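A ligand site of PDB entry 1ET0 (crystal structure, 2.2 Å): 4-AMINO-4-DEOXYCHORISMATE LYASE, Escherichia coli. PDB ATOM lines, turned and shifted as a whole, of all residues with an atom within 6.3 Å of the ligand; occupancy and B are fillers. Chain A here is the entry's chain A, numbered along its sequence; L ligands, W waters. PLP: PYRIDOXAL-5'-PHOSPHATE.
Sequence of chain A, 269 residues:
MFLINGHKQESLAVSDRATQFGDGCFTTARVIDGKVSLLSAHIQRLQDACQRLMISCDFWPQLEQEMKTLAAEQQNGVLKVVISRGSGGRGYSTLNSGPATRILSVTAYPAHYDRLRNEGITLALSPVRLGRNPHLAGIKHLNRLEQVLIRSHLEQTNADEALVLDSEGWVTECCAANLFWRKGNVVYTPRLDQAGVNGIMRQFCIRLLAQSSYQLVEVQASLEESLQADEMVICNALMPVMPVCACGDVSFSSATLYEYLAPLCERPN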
ATOM      1  N   PHE A  26     -19.951  11.086 -28.304  1.00  0.00           N
ATOM      2  CA  PHE A  26     -21.294  10.537 -28.174  1.00  0.00           C
ATOM      3  C   PHE A  26     -22.215  11.403 -27.320  1.00  0.00           C
ATOM      4  O   PHE A  26     -21.759  12.354 -26.680  1.00  0.00           O
ATOM      5  CB  PHE A  26     -21.220   9.109 -27.584  1.00  0.00           C
ATOM      6  CG  PHE A  26     -20.923   9.072 -26.101  1.00  0.00           C
ATOM      7  CD1 PHE A  26     -19.663   9.401 -25.611  1.00  0.00           C
ATOM      8  CD2 PHE A  26     -21.910   8.679 -25.189  1.00  0.00           C
ATOM      9  CE1 PHE A  26     -19.388   9.347 -24.239  1.00  0.00           C
ATOM     10  CE2 PHE A  26     -21.658   8.629 -23.835  1.00  0.00           C
ATOM     11  CZ  PHE A  26     -20.383   8.964 -23.348  1.00  0.00           C
ATOM     12  N   THR A  27     -23.504  11.078 -27.328  1.00  0.00           N
ATOM     13  CA  THR A  27     -24.483  11.800 -26.509  1.00  0.00           C
ATOM     14  C   THR A  27     -25.614  10.868 -26.147  1.00  0.00           C
ATOM     15  O   THR A  27     -25.968   9.994 -26.939  1.00  0.00           O
ATOM     16  CB  THR A  27     -25.072  13.066 -27.231  1.00  0.00           C
ATOM     17  OG1 THR A  27     -25.616  13.945 -26.234  1.00  0.00           O
ATOM     18  CG2 THR A  27     -26.203  12.701 -28.193  1.00  0.00           C
ATOM     19  N   THR A  28     -26.091  10.978 -24.918  1.00  0.00           N
ATOM     20  CA  THR A  28     -27.200  10.161 -24.464  1.00  0.00           C
ATOM     21  C   THR A  28     -28.362  11.078 -24.173  1.00  0.00           C
ATOM     22  O   THR A  28     -28.260  12.000 -23.356  1.00  0.00           O
ATOM     23  CB  THR A  28     -26.837   9.303 -23.238  1.00  0.00           C
ATOM     24  OG1 THR A  28     -26.186  10.112 -22.261  1.00  0.00           O
ATOM     25  CG2 THR A  28     -25.899   8.177 -23.633  1.00  0.00           C
ATOM     26  N   HIS A  42     -28.453  18.496 -28.169  1.00  0.00           N
ATOM     27  CA  HIS A  42     -27.683  17.288 -28.438  1.00  0.00           C
ATOM     28  C   HIS A  42     -26.929  17.355 -29.762  1.00  0.00           C
ATOM     29  O   HIS A  42     -25.789  16.942 -29.858  1.00  0.00           O
ATOM     30  CB  HIS A  42     -28.584  16.049 -28.349  1.00  0.00           C
ATOM     31  CG  HIS A  42     -28.989  15.713 -26.946  1.00  0.00           C
ATOM     32  ND1 HIS A  42     -28.083  15.299 -25.990  1.00  0.00           N
ATOM     33  CD2 HIS A  42     -30.187  15.735 -26.332  1.00  0.00           C
ATOM     34  CE1 HIS A  42     -28.700  15.084 -24.857  1.00  0.00           C
ATOM     35  NE2 HIS A  42     -29.986  15.344 -25.027  1.00  0.00           N
ATOM     36  N   ARG A  45     -23.947  19.846 -29.360  1.00  0.00           N
ATOM     37  CA  ARG A  45     -22.853  19.341 -28.547  1.00  0.00           C
ATOM     38  C   ARG A  45     -22.045  18.306 -29.371  1.00  0.00           C
ATOM     39  O   ARG A  45     -20.849  18.100 -29.142  1.00  0.00           O
ATOM     40  CB  ARG A  45     -23.358  18.741 -27.218  1.00  0.00           C
ATOM     41  CG  ARG A  45     -23.950  17.338 -27.270  1.00  0.00           C
ATOM     42  CD  ARG A  45     -23.034  16.288 -26.623  1.00  0.00           C
ATOM     43  NE  ARG A  45     -22.625  16.642 -25.265  1.00  0.00           N
ATOM     44  CZ  ARG A  45     -23.243  16.258 -24.152  1.00  0.00           C
ATOM     45  NH1 ARG A  45     -24.313  15.478 -24.212  1.00  0.00           N
ATOM     46  NH2 ARG A  45     -22.786  16.644 -22.973  1.00  0.00           N
ATOM     47  N   LYS A 140     -17.563  15.360 -24.841  1.00  0.00           N
ATOM     48  CA  LYS A 140     -18.122  14.069 -24.439  1.00  0.00           C
ATOM     49  C   LYS A 140     -17.575  13.044 -25.450  1.00  0.00           C
ATOM     50  O   LYS A 140     -18.314  12.507 -26.285  1.00  0.00           O
ATOM     51  CB  LYS A 140     -19.656  14.097 -24.480  1.00  0.00           C
ATOM     52  CG  LYS A 140     -20.331  12.956 -23.711  1.00  0.00           C
ATOM     53  CD  LYS A 140     -21.846  13.032 -23.736  1.00  0.00           C
ATOM     54  CE  LYS A 140     -22.427  12.092 -22.696  1.00  0.00           C
ATOM     55  NZ  LYS A 140     -21.756  12.431 -21.451  1.00  0.00           N
ATOM     56  N   ARG A 144     -13.621   7.142 -22.103  1.00  0.00           N
ATOM     57  CA  ARG A 144     -14.253   7.216 -20.788  1.00  0.00           C
ATOM     58  C   ARG A 144     -13.788   6.147 -19.824  1.00  0.00           C
ATOM     59  O   ARG A 144     -14.559   5.679 -18.994  1.00  0.00           O
ATOM     60  CB  ARG A 144     -15.775   7.149 -20.934  1.00  0.00           C
ATOM     61  CG  ARG A 144     -16.336   8.147 -21.932  1.00  0.00           C
ATOM     62  CD  ARG A 144     -16.727   9.486 -21.305  1.00  0.00           C
ATOM     63  NE  ARG A 144     -15.616  10.270 -20.752  1.00  0.00           N
ATOM     64  CZ  ARG A 144     -15.250  11.466 -21.189  1.00  0.00           C
ATOM     65  NH1 ARG A 144     -15.877  12.036 -22.203  1.00  0.00           N
ATOM     66  NH2 ARG A 144     -14.303  12.143 -20.552  1.00  0.00           N
ATOM     67  N   GLN A 147     -13.976   7.152 -16.160  1.00  0.00           N
ATOM     68  CA  GLN A 147     -15.337   6.963 -15.629  1.00  0.00           C
ATOM     69  C   GLN A 147     -15.610   5.497 -15.306  1.00  0.00           C
ATOM     70  O   GLN A 147     -16.356   5.203 -14.366  1.00  0.00           O
ATOM     71  CB  GLN A 147     -16.409   7.493 -16.596  1.00  0.00           C
ATOM     72  CG  GLN A 147     -16.548   9.001 -16.595  1.00  0.00           C
ATOM     73  CD  GLN A 147     -15.297   9.697 -17.127  1.00  0.00           C
ATOM     74  OE1 GLN A 147     -14.700   9.263 -18.100  1.00  0.00           O
ATOM     75  NE2 GLN A 147     -14.897  10.784 -16.472  1.00  0.00           N
ATOM     76  N   GLU A 173     -16.539  17.201 -10.916  1.00  0.00           N
ATOM     77  CA  GLU A 173     -17.883  16.714 -11.166  1.00  0.00           C
ATOM     78  C   GLU A 173     -18.110  15.392 -10.463  1.00  0.00           C
ATOM     79  O   GLU A 173     -17.512  15.133  -9.424  1.00  0.00           O
ATOM     80  CB  GLU A 173     -18.156  16.566 -12.673  1.00  0.00           C
ATOM     81  CG  GLU A 173     -17.230  15.612 -13.409  1.00  0.00           C
ATOM     82  CD  GLU A 173     -17.872  15.077 -14.685  1.00  0.00           C
ATOM     83  OE1 GLU A 173     -18.756  14.205 -14.580  1.00  0.00           O
ATOM     84  OE2 GLU A 173     -17.499  15.538 -15.776  1.00  0.00           O
ATOM     85  N   CYS A 174     -19.052  14.609 -10.982  1.00  0.00           N
ATOM     86  CA  CYS A 174     -19.383  13.298 -10.437  1.00  0.00           C
ATOM     87  C   CYS A 174     -18.929  12.283 -11.487  1.00  0.00           C
ATOM     88  O   CYS A 174     -18.191  12.636 -12.400  1.00  0.00           O
ATOM     89  CB  CYS A 174     -20.894  13.182 -10.189  1.00  0.00           C
ATOM     90  SG  CYS A 174     -21.556  14.350  -8.983  1.00  0.00           S
ATOM     91  N   CYS A 175     -19.375  11.030 -11.365  1.00  0.00           N
ATOM     92  CA  CYS A 175     -18.976  10.026 -12.336  1.00  0.00           C
ATOM     93  C   CYS A 175     -19.655  10.227 -13.691  1.00  0.00           C
ATOM     94  O   CYS A 175     -18.984  10.229 -14.743  1.00  0.00           O
ATOM     95  CB  CYS A 175     -19.287   8.617 -11.804  1.00  0.00           C
ATOM     96  SG  CYS A 175     -18.827   7.287 -12.955  1.00  0.00           S
ATOM     97  N   ALA A 176     -20.966  10.435 -13.677  1.00  0.00           N
ATOM     98  CA  ALA A 176     -21.728  10.612 -14.897  1.00  0.00           C
ATOM     99  C   ALA A 176     -22.718  11.781 -14.812  1.00  0.00           C
ATOM    100  O   ALA A 176     -23.760  11.797 -15.489  1.00  0.00           O
ATOM    101  CB  ALA A 176     -22.473   9.311 -15.212  1.00  0.00           C
ATOM    102  N   ALA A 177     -22.379  12.783 -14.009  1.00  0.00           N
ATOM    103  CA  ALA A 177     -23.230  13.953 -13.835  1.00  0.00           C
ATOM    104  C   ALA A 177     -22.408  15.165 -13.390  1.00  0.00           C
ATOM    105  O   ALA A 177     -21.289  15.038 -12.897  1.00  0.00           O
ATOM    106  CB  ALA A 177     -24.331  13.644 -12.811  1.00  0.00           C
ATOM    107  N   ASN A 178     -22.955  16.359 -13.621  1.00  0.00           N
ATOM    108  CA  ASN A 178     -22.282  17.588 -13.230  1.00  0.00           C
ATOM    109  C   ASN A 178     -22.734  17.978 -11.838  1.00  0.00           C
ATOM    110  O   ASN A 178     -23.726  17.472 -11.320  1.00  0.00           O
ATOM    111  CB  ASN A 178     -22.559  18.703 -14.250  1.00  0.00           C
ATOM    112  CG  ASN A 178     -21.868  18.441 -15.579  1.00  0.00           C
ATOM    113  OD1 ASN A 178     -22.527  18.158 -16.586  1.00  0.00           O
ATOM    114  ND2 ASN A 178     -20.552  18.547 -15.593  1.00  0.00           N
ATOM    115  N   GLY A 196     -13.423  17.012 -17.066  1.00  0.00           N
ATOM    116  CA  GLY A 196     -14.864  16.835 -17.032  1.00  0.00           C
ATOM    117  C   GLY A 196     -15.590  17.122 -18.327  1.00  0.00           C
ATOM    118  O   GLY A 196     -15.024  17.641 -19.281  1.00  0.00           O
ATOM    119  N   VAL A 197     -16.872  16.756 -18.362  1.00  0.00           N
ATOM    120  CA  VAL A 197     -17.709  16.976 -19.540  1.00  0.00           C
ATOM    121  C   VAL A 197     -18.691  18.107 -19.260  1.00  0.00           C
ATOM    122  O   VAL A 197     -19.333  18.153 -18.214  1.00  0.00           O
ATOM    123  CB  VAL A 197     -18.504  15.699 -19.906  1.00  0.00           C
ATOM    124  CG1 VAL A 197     -19.429  15.970 -21.102  1.00  0.00           C
ATOM    125  CG2 VAL A 197     -17.547  14.553 -20.231  1.00  0.00           C
ATOM    126  N   ASN A 198     -18.781  19.034 -20.197  1.00  0.00           N
ATOM    127  CA  ASN A 198     -19.700  20.158 -20.068  1.00  0.00           C
ATOM    128  C   ASN A 198     -21.105  19.695 -20.476  1.00  0.00           C
ATOM    129  O   ASN A 198     -21.539  19.874 -21.619  1.00  0.00           O
ATOM    130  CB  ASN A 198     -19.251  21.302 -20.979  1.00  0.00           C
ATOM    131  CG  ASN A 198     -20.013  22.563 -20.720  1.00  0.00           C
ATOM    132  OD1 ASN A 198     -20.881  22.616 -19.851  1.00  0.00           O
ATOM    133  ND2 ASN A 198     -19.705  23.605 -21.471  1.00  0.00           N
ATOM    134  N   GLY A 199     -21.805  19.074 -19.528  1.00  0.00           N
ATOM    135  CA  GLY A 199     -23.133  18.558 -19.793  1.00  0.00           C
ATOM    136  C   GLY A 199     -24.176  19.492 -20.390  1.00  0.00           C
ATOM    137  O   GLY A 199     -24.121  20.712 -20.209  1.00  0.00           O
ATOM    138  N   ILE A 200     -25.136  18.881 -21.085  1.00  0.00           N
ATOM    139  CA  ILE A 200     -26.238  19.576 -21.749  1.00  0.00           C
ATOM    140  C   ILE A 200     -27.243  20.085 -20.696  1.00  0.00           C
ATOM    141  O   ILE A 200     -27.870  21.124 -20.888  1.00  0.00           O
ATOM    142  CB  ILE A 200     -26.945  18.652 -22.792  1.00  0.00           C
ATOM    143  CG1 ILE A 200     -27.008  19.346 -24.136  1.00  0.00           C
ATOM    144  CG2 ILE A 200     -28.355  18.248 -22.359  1.00  0.00           C
ATOM    145  CD1 ILE A 200     -25.668  19.660 -24.698  1.00  0.00           C
ATOM    146  N   MET A 201     -27.388  19.326 -19.615  1.00  0.00           N
ATOM    147  CA  MET A 201     -28.295  19.703 -18.548  1.00  0.00           C
ATOM    148  C   MET A 201     -27.648  20.795 -17.712  1.00  0.00           C
ATOM    149  O   MET A 201     -28.337  21.649 -17.159  1.00  0.00           O
ATOM    150  CB  MET A 201     -28.633  18.513 -17.658  1.00  0.00           C
ATOM    151  CG  MET A 201     -29.794  18.787 -16.717  1.00  0.00           C
ATOM    152  SD  MET A 201     -31.180  19.506 -17.630  1.00  0.00           S
ATOM    153  CE  MET A 201     -31.681  18.114 -18.687  1.00  0.00           C
ATOM    154  N   ARG A 202     -26.310  20.749 -17.637  1.00  0.00           N
ATOM    155  CA  ARG A 202     -25.517  21.715 -16.906  1.00  0.00           C
ATOM    156  C   ARG A 202     -25.698  23.075 -17.557  1.00  0.00           C
ATOM    157  O   ARG A 202     -26.024  24.055 -16.887  1.00  0.00           O
ATOM    158  CB  ARG A 202     -24.046  21.331 -16.955  1.00  0.00           C
ATOM    159  CG  ARG A 202     -23.111  22.436 -16.485  1.00  0.00           C
ATOM    160  CD  ARG A 202     -21.658  22.042 -16.638  1.00  0.00           C
ATOM    161  NE  ARG A 202     -20.734  22.989 -16.017  1.00  0.00           N
ATOM    162  CZ  ARG A 202     -20.374  24.140 -16.580  1.00  0.00           C
ATOM    163  NH1 ARG A 202     -20.850  24.488 -17.768  1.00  0.00           N
ATOM    164  NH2 ARG A 202     -19.539  24.960 -15.942  1.00  0.00           N
ATOM    165  N   GLN A 203     -25.477  23.118 -18.866  1.00  0.00           N
ATOM    166  CA  GLN A 203     -25.622  24.344 -19.616  1.00  0.00           C
ATOM    167  C   GLN A 203     -27.057  24.862 -19.585  1.00  0.00           C
ATOM    168  O   GLN A 203     -27.282  26.067 -19.616  1.00  0.00           O
ATOM    169  CB  GLN A 203     -25.185  24.130 -21.064  1.00  0.00           C
ATOM    170  CG  GLN A 203     -23.796  23.535 -21.206  1.00  0.00           C
ATOM    171  CD  GLN A 203     -23.401  23.388 -22.658  1.00  0.00           C
ATOM    172  OE1 GLN A 203     -23.344  24.367 -23.402  1.00  0.00           O
ATOM    173  NE2 GLN A 203     -23.154  22.145 -23.085  1.00  0.00           N
ATOM    174  N   CYS A 235     -26.748  16.709 -11.744  1.00  0.00           N
ATOM    175  CA  CYS A 235     -27.537  16.751 -12.984  1.00  0.00           C
ATOM    176  C   CYS A 235     -26.943  16.092 -14.239  1.00  0.00           C
ATOM    177  O   CYS A 235     -25.737  15.943 -14.363  1.00  0.00           O
ATOM    178  CB  CYS A 235     -27.882  18.215 -13.332  1.00  0.00           C
ATOM    179  SG  CYS A 235     -26.532  19.231 -14.020  1.00  0.00           S
ATOM    180  N   ASN A 236     -27.842  15.709 -15.146  1.00  0.00           N
ATOM    181  CA  ASN A 236     -27.516  15.122 -16.455  1.00  0.00           C
ATOM    182  C   ASN A 236     -28.794  15.012 -17.295  1.00  0.00           C
ATOM    183  O   ASN A 236     -29.897  15.165 -16.770  1.00  0.00           O
ATOM    184  CB  ASN A 236     -26.734  13.795 -16.356  1.00  0.00           C
ATOM    185  CG  ASN A 236     -27.598  12.609 -15.996  1.00  0.00           C
ATOM    186  OD1 ASN A 236     -28.789  12.565 -16.279  1.00  0.00           O
ATOM    187  ND2 ASN A 236     -26.981  11.600 -15.411  1.00  0.00           N
ATOM    188  N   ALA A 237     -28.662  14.737 -18.585  1.00  0.00           N
ATOM    189  CA  ALA A 237     -29.794  14.628 -19.501  1.00  0.00           C
ATOM    190  C   ALA A 237     -30.882  13.625 -19.099  1.00  0.00           C
ATOM    191  O   ALA A 237     -32.067  13.824 -19.408  1.00  0.00           O
ATOM    192  CB  ALA A 237     -29.292  14.305 -20.917  1.00  0.00           C
ATOM    193  N   LEU A 238     -30.491  12.559 -18.403  1.00  0.00           N
ATOM    194  CA  LEU A 238     -31.424  11.521 -17.998  1.00  0.00           C
ATOM    195  C   LEU A 238     -32.135  11.631 -16.645  1.00  0.00           C
ATOM    196  O   LEU A 238     -33.224  11.071 -16.498  1.00  0.00           O
ATOM    197  CB  LEU A 238     -30.760  10.132 -18.102  1.00  0.00           C
ATOM    198  CG  LEU A 238     -30.173   9.626 -19.428  1.00  0.00           C
ATOM    199  CD1 LEU A 238     -31.113   9.886 -20.586  1.00  0.00           C
ATOM    200  CD2 LEU A 238     -28.862  10.318 -19.696  1.00  0.00           C
HETATM  201  N1  PLP L   1     -20.278  13.722 -16.784  1.00  0.00           N
HETATM  202  C2  PLP L   1     -19.742  12.812 -17.664  1.00  0.00           C
HETATM  203  C2A PLP L   1     -18.368  12.175 -17.353  1.00  0.00           C
HETATM  204  C3  PLP L   1     -20.422  12.477 -18.794  1.00  0.00           C
HETATM  205  O3  PLP L   1     -19.896  11.571 -19.687  1.00  0.00           O
HETATM  206  C4  PLP L   1     -21.671  13.073 -19.027  1.00  0.00           C
HETATM  207  C4A PLP L   1     -22.443  12.692 -20.301  1.00  0.00           C
HETATM  208  C5  PLP L   1     -22.193  13.998 -18.093  1.00  0.00           C
HETATM  209  C6  PLP L   1     -21.485  14.305 -16.987  1.00  0.00           C
HETATM  210  C5A PLP L   1     -23.552  14.641 -18.292  1.00  0.00           C
HETATM  211  O4P PLP L   1     -23.863  15.153 -19.559  1.00  0.00           O
HETATM  212  P   PLP L   1     -25.279  15.711 -19.918  1.00  0.00           P
HETATM  213  O1P PLP L   1     -26.151  14.530 -19.893  1.00  0.00           O
HETATM  214  O2P PLP L   1     -24.988  16.164 -21.405  1.00  0.00           O
HETATM  215  O3P PLP L   1     -25.633  16.846 -19.079  1.00  0.00           O
HETATM  216  O   HOH W   1     -24.331  10.613 -18.223  1.00  0.00           O
HETATM  217  O   HOH W   2     -26.316  11.887 -19.803  1.00  0.00           O
HETATM  218  O   HOH W   3     -25.971  13.458 -22.667  1.00  0.00           O
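A carbon (C4A) of the ligand is bonded to the side-chain amino group (NZ) of Lys 140, 1.4 Å away.
A nitrogen (N1) of the ligand sits at hydrogen-bond distance from the side-chain carboxylate of Glu 173 (2.7 Å).
The backbone NH (N) of Ile 200 is in hydrogen-bond range of an oxygen (O2P) of the ligand, 2.7 Å away.
The guanidinium group (NH2) of Arg 45 lies within salt-bridge range of an oxygen (O2P) of the ligand.
An oxygen (O1P) of the ligand is in hydrogen-bond range of the backbone NH (N) of Ala 237 (2.8 Å).
N of Met 201 is in hydrogen-bond range of O3P of the ligand.
The backbone carbonyl oxygen of Lys 140 is in hydrogen-bond range of the backbone NH of Phe 26.
OE2 of Glu 173 is in hydrogen-bond range of N of Val 197.
The guanidinium group (NH1) of Arg 45 is in hydrogen-bond range of the side-chain hydroxyl (OG1) of Thr 27.
The backbone NH (N) of Gly 199 lies within hydrogen-bond range of the side-chain amide oxygen (OD1) of Asn 178 (3.2 Å).
The side-chain sulfur (SG) of Cys 175 sits at hydrogen-bond distance from the backbone carbonyl oxygen (O) of Gln 147, at 3.5 Å.
The backbone NH (N) of Leu 238 sits at hydrogen-bond distance from the side-chain amide oxygen (OD1) of Asn 236 (2.7 Å).
The side-chain amide oxygen (OE1) of Gln 147 lies within hydrogen-bond range of the guanidinium group (NE) of Arg 144 (3.0 Å).
The side-chain amide nitrogen (ND2) of Asn 178 is in hydrogen-bond range of the backbone carbonyl oxygen (O) of Val 197, at 2.9 Å.
Merely in contact with the ligand: Gln 147 (3.7 Å), Cys 175 (3.3 Å), Ala 176 (3.6 Å), Ala 177 (3.5 Å), Val 197 (3.8 Å), Gly 199 (3.1 Å) and Asn 236 (3.7 Å).
Hydrophobic or aromatic side chains that line the ligand: Val 197, Ile 200, Met 201 and Ala 237.
Along chain A the residues within 4 Å of the ligand span positions 45 to 237.
The nearest printed residue that does not touch the ligand is Asn 178 (4.01 Å).
Water W2 bridges an oxygen (O1P) of the ligand (2.6 Å) and the side-chain hydroxyl (OG1) of Thr 28 (3.0 Å).
Water W3 lies within hydrogen-bond range of O of Thr 28 (2.8 Å), O1P of the ligand (3.0 Å) and NH1 of Arg 45 (3.0 Å).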
